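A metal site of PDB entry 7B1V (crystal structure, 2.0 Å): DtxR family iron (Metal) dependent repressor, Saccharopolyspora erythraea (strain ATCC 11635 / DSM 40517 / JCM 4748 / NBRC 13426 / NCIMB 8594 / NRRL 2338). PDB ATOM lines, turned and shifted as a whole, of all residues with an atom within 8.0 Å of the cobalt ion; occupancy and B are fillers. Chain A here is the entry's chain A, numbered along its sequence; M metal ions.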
ATOM      1  N   ARG A  15      -8.384  -2.486  13.475  1.00  0.00           N
ATOM      2  CA  ARG A  15      -8.064  -2.211  12.050  1.00  0.00           C
ATOM      3  C   ARG A  15      -7.361  -3.413  11.424  1.00  0.00           C
ATOM      4  O   ARG A  15      -7.571  -3.634  10.210  1.00  0.00           O
ATOM      5  CB  ARG A  15      -7.222  -0.941  11.908  1.00  0.00           C
ATOM      6  CG  ARG A  15      -7.459  -0.192  10.596  1.00  0.00           C
ATOM      7  CD  ARG A  15      -6.229   0.553  10.132  1.00  0.00           C
ATOM      8  NE  ARG A  15      -5.244  -0.356   9.549  1.00  0.00           N
ATOM      9  CZ  ARG A  15      -3.995  -0.016   9.227  1.00  0.00           C
ATOM     10  NH1 ARG A  15      -3.561   1.217   9.444  1.00  0.00           N
ATOM     11  NH2 ARG A  15      -3.180  -0.906   8.704  1.00  0.00           N
ATOM     12  N   ASP A  19      -8.366  -5.319   8.235  1.00  0.00           N
ATOM     13  CA  ASP A  19      -7.324  -5.543   7.182  1.00  0.00           C
ATOM     14  C   ASP A  19      -7.406  -6.994   6.694  1.00  0.00           C
ATOM     15  O   ASP A  19      -7.475  -7.205   5.472  1.00  0.00           O
ATOM     16  CB  ASP A  19      -5.923  -5.224   7.689  1.00  0.00           C
ATOM     17  CG  ASP A  19      -5.595  -3.748   7.812  1.00  0.00           C
ATOM     18  OD1 ASP A  19      -6.263  -2.932   7.144  1.00  0.00           O
ATOM     19  OD2 ASP A  19      -4.675  -3.412   8.594  1.00  0.00           O
ATOM     20  N   MET A  78      -9.794   3.355   9.657  1.00  0.00           N
ATOM     21  CA  MET A  78      -9.382   3.103   8.257  1.00  0.00           C
ATOM     22  C   MET A  78      -9.645   4.350   7.405  1.00  0.00           C
ATOM     23  O   MET A  78      -8.773   4.705   6.583  1.00  0.00           O
ATOM     24  CB  MET A  78     -10.151   1.922   7.648  1.00  0.00           C
ATOM     25  CG  MET A  78      -9.576   1.442   6.326  1.00  0.00           C
ATOM     26  SD  MET A  78      -8.070   0.462   6.533  1.00  0.00           S
ATOM     27  CE  MET A  78      -6.811   1.716   6.366  1.00  0.00           C
ATOM     28  N   HIS A  81      -7.069   6.980   8.246  1.00  0.00           N
ATOM     29  CA  HIS A  81      -5.804   6.445   7.656  1.00  0.00           C
ATOM     30  C   HIS A  81      -5.713   6.834   6.177  1.00  0.00           C
ATOM     31  O   HIS A  81      -4.684   7.411   5.786  1.00  0.00           O
ATOM     32  CB  HIS A  81      -5.726   4.923   7.850  1.00  0.00           C
ATOM     33  CG  HIS A  81      -4.487   4.296   7.302  1.00  0.00           C
ATOM     34  ND1 HIS A  81      -3.329   4.189   8.045  1.00  0.00           N
ATOM     35  CD2 HIS A  81      -4.235   3.721   6.105  1.00  0.00           C
ATOM     36  CE1 HIS A  81      -2.409   3.586   7.316  1.00  0.00           C
ATOM     37  NE2 HIS A  81      -2.936   3.291   6.126  1.00  0.00           N
ATOM     38  N   ARG A  82      -6.762   6.541   5.408  1.00  0.00           N
ATOM     39  CA  ARG A  82      -6.749   6.656   3.922  1.00  0.00           C
ATOM     40  C   ARG A  82      -6.939   8.118   3.511  1.00  0.00           C
ATOM     41  O   ARG A  82      -6.316   8.526   2.518  1.00  0.00           O
ATOM     42  CB  ARG A  82      -7.771   5.677   3.320  1.00  0.00           C
ATOM     43  CG  ARG A  82      -7.335   4.229   3.449  1.00  0.00           C
ATOM     44  CD  ARG A  82      -8.347   3.187   3.042  1.00  0.00           C
ATOM     45  NE  ARG A  82      -7.752   1.860   3.086  1.00  0.00           N
ATOM     46  CZ  ARG A  82      -8.400   0.705   3.032  1.00  0.00           C
ATOM     47  NH1 ARG A  82      -9.722   0.674   2.910  1.00  0.00           N
ATOM     48  NH2 ARG A  82      -7.725  -0.429   3.092  1.00  0.00           N
ATOM     49  N   GLU A  85      -3.543   9.482   4.088  1.00  0.00           N
ATOM     50  CA  GLU A  85      -2.629   9.014   3.002  1.00  0.00           C
ATOM     51  C   GLU A  85      -2.785   9.921   1.769  1.00  0.00           C
ATOM     52  O   GLU A  85      -1.742  10.272   1.174  1.00  0.00           O
ATOM     53  CB  GLU A  85      -2.922   7.552   2.654  1.00  0.00           C
ATOM     54  CG  GLU A  85      -2.368   6.569   3.682  1.00  0.00           C
ATOM     55  CD  GLU A  85      -2.577   5.109   3.333  1.00  0.00           C
ATOM     56  OE1 GLU A  85      -3.568   4.788   2.643  1.00  0.00           O
ATOM     57  OE2 GLU A  85      -1.747   4.279   3.750  1.00  0.00           O
ATOM     58  N   VAL A  99       4.499   7.063   3.263  1.00  0.00           N
ATOM     59  CA  VAL A  99       3.196   7.706   3.604  1.00  0.00           C
ATOM     60  C   VAL A  99       2.389   6.809   4.556  1.00  0.00           C
ATOM     61  O   VAL A  99       1.754   7.368   5.476  1.00  0.00           O
ATOM     62  CB  VAL A  99       2.403   8.077   2.329  1.00  0.00           C
ATOM     63  CG1 VAL A  99       0.898   8.064   2.553  1.00  0.00           C
ATOM     64  CG2 VAL A  99       2.852   9.429   1.781  1.00  0.00           C
ATOM     65  N   HIS A 100       2.381   5.494   4.338  1.00  0.00           N
ATOM     66  CA  HIS A 100       1.583   4.522   5.149  1.00  0.00           C
ATOM     67  C   HIS A 100       2.054   4.527   6.605  1.00  0.00           C
ATOM     68  O   HIS A 100       1.188   4.503   7.497  1.00  0.00           O
ATOM     69  CB  HIS A 100       1.648   3.107   4.569  1.00  0.00           C
ATOM     70  CG  HIS A 100       1.107   2.069   5.488  1.00  0.00           C
ATOM     71  ND1 HIS A 100      -0.260   1.868   5.642  1.00  0.00           N
ATOM     72  CD2 HIS A 100       1.713   1.197   6.320  1.00  0.00           C
ATOM     73  CE1 HIS A 100      -0.457   0.912   6.529  1.00  0.00           C
ATOM     74  NE2 HIS A 100       0.737   0.486   6.949  1.00  0.00           N
ATOM     75  N   LEU A 101       3.371   4.527   6.819  1.00  0.00           N
ATOM     76  CA  LEU A 101       4.005   4.528   8.164  1.00  0.00           C
ATOM     77  C   LEU A 101       3.500   5.752   8.947  1.00  0.00           C
ATOM     78  O   LEU A 101       3.176   5.595  10.144  1.00  0.00           O
ATOM     79  CB  LEU A 101       5.532   4.546   8.034  1.00  0.00           C
ATOM     80  CG  LEU A 101       6.198   3.184   7.836  1.00  0.00           C
ATOM     81  CD1 LEU A 101       5.787   2.549   6.514  1.00  0.00           C
ATOM     82  CD2 LEU A 101       7.709   3.305   7.912  1.00  0.00           C
ATOM     83  N   GLU A 102       3.417   6.903   8.271  1.00  0.00           N
ATOM     84  CA  GLU A 102       2.938   8.191   8.846  1.00  0.00           C
ATOM     85  C   GLU A 102       1.442   8.078   9.156  1.00  0.00           C
ATOM     86  O   GLU A 102       1.039   8.476  10.274  1.00  0.00           O
ATOM     87  CB  GLU A 102       3.207   9.332   7.864  1.00  0.00           C
ATOM     88  CG  GLU A 102       3.143  10.708   8.489  1.00  0.00           C
ATOM     89  CD  GLU A 102       4.332  11.077   9.370  1.00  0.00           C
ATOM     90  OE1 GLU A 102       5.408  10.485   9.183  1.00  0.00           O
ATOM     91  OE2 GLU A 102       4.183  11.969  10.217  1.00  0.00           O
ATOM     92  N   ALA A 103       0.654   7.546   8.218  1.00  0.00           N
ATOM     93  CA  ALA A 103      -0.812   7.376   8.310  1.00  0.00           C
ATOM     94  C   ALA A 103      -1.185   6.402   9.421  1.00  0.00           C
ATOM     95  O   ALA A 103      -2.268   6.496  10.013  1.00  0.00           O
ATOM     96  CB  ALA A 103      -1.356   6.919   6.971  1.00  0.00           C
ATOM     97  N   CSD A 104      -0.281   5.452   9.696  1.00  0.00           N
ATOM     98  CA  CSD A 104      -0.470   4.459  10.748  1.00  0.00           C
ATOM     99  CB  CSD A 104       0.634   3.402  10.717  1.00  0.00           C
ATOM    100  SG  CSD A 104      -0.091   1.742  10.789  1.00  0.00           S
ATOM    101  C   CSD A 104      -0.561   5.122  12.120  1.00  0.00           C
ATOM    102  O   CSD A 104      -1.194   4.588  13.020  1.00  0.00           O
ATOM    103  OD1 CSD A 104       1.030   0.808  10.535  1.00  0.00           O
ATOM    104  OD2 CSD A 104      -0.575   1.513  12.296  1.00  0.00           O
ATOM    105  N   GLU A 107      -3.865   8.227  11.907  1.00  0.00           N
ATOM    106  CA  GLU A 107      -5.228   7.626  11.933  1.00  0.00           C
ATOM    107  C   GLU A 107      -5.818   7.651  13.356  1.00  0.00           C
ATOM    108  O   GLU A 107      -7.049   7.654  13.470  1.00  0.00           O
ATOM    109  CB  GLU A 107      -5.198   6.196  11.381  1.00  0.00           C
ATOM    110  CG  GLU A 107      -4.327   5.235  12.183  1.00  0.00           C
ATOM    111  CD  GLU A 107      -4.150   3.861  11.557  1.00  0.00           C
ATOM    112  OE1 GLU A 107      -4.936   3.518  10.648  1.00  0.00           O
ATOM    113  OE2 GLU A 107      -3.238   3.137  11.982  1.00  0.00           O
ATOM    114  N   SER A 128      -7.766   5.465  -1.475  1.00  0.00           N
ATOM    115  CA  SER A 128      -6.433   5.894  -0.979  1.00  0.00           C
ATOM    116  C   SER A 128      -5.476   5.964  -2.175  1.00  0.00           C
ATOM    117  O   SER A 128      -5.828   5.514  -3.264  1.00  0.00           O
ATOM    118  CB  SER A 128      -5.923   4.975   0.104  1.00  0.00           C
ATOM    119  OG  SER A 128      -5.334   3.797  -0.446  1.00  0.00           O
ATOM    120  N   PRO A 129      -4.260   6.528  -2.019  1.00  0.00           N
ATOM    121  CA  PRO A 129      -3.274   6.537  -3.097  1.00  0.00           C
ATOM    122  C   PRO A 129      -2.841   5.132  -3.547  1.00  0.00           C
ATOM    123  O   PRO A 129      -2.212   5.028  -4.579  1.00  0.00           O
ATOM    124  CB  PRO A 129      -2.062   7.284  -2.500  1.00  0.00           C
ATOM    125  CG  PRO A 129      -2.645   8.081  -1.355  1.00  0.00           C
ATOM    126  CD  PRO A 129      -3.780   7.227  -0.815  1.00  0.00           C
ATOM    127  N   TYR A 130      -3.171   4.110  -2.751  1.00  0.00           N
ATOM    128  CA  TYR A 130      -2.842   2.674  -3.002  1.00  0.00           C
ATOM    129  C   TYR A 130      -4.083   1.931  -3.517  1.00  0.00           C
ATOM    130  O   TYR A 130      -4.070   0.685  -3.521  1.00  0.00           O
ATOM    131  CB  TYR A 130      -2.249   2.066  -1.726  1.00  0.00           C
ATOM    132  CG  TYR A 130      -1.188   2.928  -1.105  1.00  0.00           C
ATOM    133  CD1 TYR A 130       0.089   2.980  -1.644  1.00  0.00           C
ATOM    134  CD2 TYR A 130      -1.454   3.726  -0.007  1.00  0.00           C
ATOM    135  CE1 TYR A 130       1.074   3.777  -1.090  1.00  0.00           C
ATOM    136  CE2 TYR A 130      -0.484   4.533   0.556  1.00  0.00           C
ATOM    137  CZ  TYR A 130       0.787   4.562   0.010  1.00  0.00           C
ATOM    138  OH  TYR A 130       1.750   5.353   0.560  1.00  0.00           O
ATOM    139  N   ASN A 132      -7.109   1.498  -2.456  1.00  0.00           N
ATOM    140  CA  ASN A 132      -8.052   0.918  -1.467  1.00  0.00           C
ATOM    141  C   ASN A 132      -9.203   1.890  -1.259  1.00  0.00           C
ATOM    142  O   ASN A 132      -8.973   3.082  -1.032  1.00  0.00           O
ATOM    143  CB  ASN A 132      -7.374   0.592  -0.138  1.00  0.00           C
ATOM    144  CG  ASN A 132      -6.251  -0.410  -0.267  1.00  0.00           C
ATOM    145  OD1 ASN A 132      -6.462  -1.531  -0.721  1.00  0.00           O
ATOM    146  ND2 ASN A 132      -5.057  -0.031   0.152  1.00  0.00           N
ATOM    147  N   ILE A 172      -3.537  -2.223  -3.435  1.00  0.00           N
ATOM    148  CA  ILE A 172      -2.409  -2.760  -2.623  1.00  0.00           C
ATOM    149  C   ILE A 172      -2.804  -2.631  -1.143  1.00  0.00           C
ATOM    150  O   ILE A 172      -2.905  -1.480  -0.667  1.00  0.00           O
ATOM    151  CB  ILE A 172      -1.087  -2.015  -2.919  1.00  0.00           C
ATOM    152  CG1 ILE A 172      -0.700  -2.105  -4.392  1.00  0.00           C
ATOM    153  CG2 ILE A 172       0.033  -2.508  -2.017  1.00  0.00           C
ATOM    154  CD1 ILE A 172       0.346  -1.090  -4.819  1.00  0.00           C
ATOM    155  N   ALA A 173      -3.033  -3.755  -0.463  1.00  0.00           N
ATOM    156  CA  ALA A 173      -3.558  -3.801   0.925  1.00  0.00           C
ATOM    157  C   ALA A 173      -2.538  -3.207   1.896  1.00  0.00           C
ATOM    158  O   ALA A 173      -1.339  -3.139   1.543  1.00  0.00           O
ATOM    159  CB  ALA A 173      -3.892  -5.228   1.302  1.00  0.00           C
ATOM    160  N   GLU A 174      -3.005  -2.805   3.084  1.00  0.00           N
ATOM    161  CA  GLU A 174      -2.215  -2.090   4.124  1.00  0.00           C
ATOM    162  C   GLU A 174      -1.016  -2.951   4.544  1.00  0.00           C
ATOM    163  O   GLU A 174       0.052  -2.382   4.812  1.00  0.00           O
ATOM    164  CB  GLU A 174      -3.097  -1.758   5.329  1.00  0.00           C
ATOM    165  CG  GLU A 174      -4.310  -0.910   4.990  1.00  0.00           C
ATOM    166  CD  GLU A 174      -4.016   0.435   4.337  1.00  0.00           C
ATOM    167  OE1 GLU A 174      -4.924   0.971   3.674  1.00  0.00           O
ATOM    168  OE2 GLU A 174      -2.891   0.933   4.492  1.00  0.00           O
ATOM    169  N   HIS A 175      -1.191  -4.287   4.587  1.00  0.00           N
ATOM    170  CA  HIS A 175      -0.165  -5.279   4.993  1.00  0.00           C
ATOM    171  C   HIS A 175       1.087  -5.142   4.121  1.00  0.00           C
ATOM    172  O   HIS A 175       2.196  -5.273   4.660  1.00  0.00           O
ATOM    173  CB  HIS A 175      -0.749  -6.695   4.966  1.00  0.00           C
ATOM    174  CG  HIS A 175       0.187  -7.736   5.503  1.00  0.00           C
ATOM    175  ND1 HIS A 175       0.387  -8.940   4.875  1.00  0.00           N
ATOM    176  CD2 HIS A 175       0.975  -7.727   6.601  1.00  0.00           C
ATOM    177  CE1 HIS A 175       1.265  -9.653   5.559  1.00  0.00           C
ATOM    178  NE2 HIS A 175       1.638  -8.929   6.631  1.00  0.00           N
ATOM    179  N   VAL A 176       0.913  -4.890   2.819  1.00  0.00           N
ATOM    180  CA  VAL A 176       2.030  -4.713   1.841  1.00  0.00           C
ATOM    181  C   VAL A 176       2.788  -3.416   2.168  1.00  0.00           C
ATOM    182  O   VAL A 176       4.025  -3.405   2.027  1.00  0.00           O
ATOM    183  CB  VAL A 176       1.516  -4.719   0.385  1.00  0.00           C
ATOM    184  CG1 VAL A 176       2.646  -4.487  -0.614  1.00  0.00           C
ATOM    185  CG2 VAL A 176       0.758  -5.986   0.043  1.00  0.00           C
ATOM    186  N   GLN A 177       2.061  -2.383   2.600  1.00  0.00           N
ATOM    187  CA  GLN A 177       2.575  -0.990   2.740  1.00  0.00           C
ATOM    188  C   GLN A 177       3.488  -0.854   3.956  1.00  0.00           C
ATOM    189  O   GLN A 177       4.160   0.193   4.061  1.00  0.00           O
ATOM    190  CB  GLN A 177       1.395  -0.015   2.834  1.00  0.00           C
ATOM    191  CG  GLN A 177       0.439  -0.085   1.649  1.00  0.00           C
ATOM    192  CD  GLN A 177      -0.786   0.762   1.859  1.00  0.00           C
ATOM    193  OE1 GLN A 177      -0.788   1.698   2.648  1.00  0.00           O
ATOM    194  NE2 GLN A 177      -1.855   0.429   1.149  1.00  0.00           N
ATOM    195  N   LEU A 178       3.532  -1.856   4.837  1.00  0.00           N
ATOM    196  CA  LEU A 178       4.421  -1.904   6.029  1.00  0.00           C
ATOM    197  C   LEU A 178       5.889  -2.088   5.599  1.00  0.00           C
ATOM    198  O   LEU A 178       6.770  -1.871   6.453  1.00  0.00           O
ATOM    199  CB  LEU A 178       3.982  -3.038   6.955  1.00  0.00           C
ATOM    200  CG  LEU A 178       2.774  -2.747   7.847  1.00  0.00           C
ATOM    201  CD1 LEU A 178       2.365  -3.989   8.616  1.00  0.00           C
ATOM    202  CD2 LEU A 178       3.050  -1.592   8.800  1.00  0.00           C
ATOM    203  N   MET A 183       7.439  -1.409  -1.469  1.00  0.00           N
ATOM    204  CA  MET A 183       6.609  -0.333  -2.057  1.00  0.00           C
ATOM    205  C   MET A 183       7.432   0.472  -3.075  1.00  0.00           C
ATOM    206  O   MET A 183       6.850   0.941  -4.064  1.00  0.00           O
ATOM    207  CB  MET A 183       6.056   0.604  -0.978  1.00  0.00           C
ATOM    208  CG  MET A 183       5.051  -0.054  -0.041  1.00  0.00           C
ATOM    209  SD  MET A 183       3.536  -0.605  -0.858  1.00  0.00           S
ATOM    210  CE  MET A 183       2.763   0.970  -1.224  1.00  0.00           C
HETATM  211 CO    CO M   1      -1.922   2.505   4.444  1.00  0.00          CO
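Within 4 Å of the cobalt ion: His 81, Glu 85, His 100, Glu 174 and Gln 177. The nearest printed residue that does not touch the cobalt ion is Tyr 130 (4.6 Å).
The side-chain carboxylate (OE2) of Glu 174 is bound to the cobalt ion, at 1.8 Å. OE2 of Glu 85 binds the cobalt ion (1.9 Å). NE2 of His 81 binds the cobalt ion. ND1 of His 100 is bound to the cobalt ion (2.1 Å). The cobalt ion is bound by the side-chain amide oxygen (OE1) of Gln 177, 2.3 Å away.
A ring nitrogen (ND1) of His 81 lies within hydrogen-bond range of the side-chain carboxylate (OE1) of Glu 107 (3.1 Å). ND2 of Asn 132 lies close to NE2 of Gln 177 (3.4 Å). The side-chain carboxylate of Glu 174 is in salt-bridge range of the guanidinium group of Arg 82 (3.0 Å). ND1 of His 81 sits at hydrogen-bond distance from NH1 of Arg 15, 3.3 Å away. The side-chain amide nitrogen of Gln 177 lies within hydrogen-bond range of the backbone carbonyl oxygen of Ile 172 (2.8 Å). ND1 of His 81 is in hydrogen-bond range of O of Ala 103 (3.2 Å).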
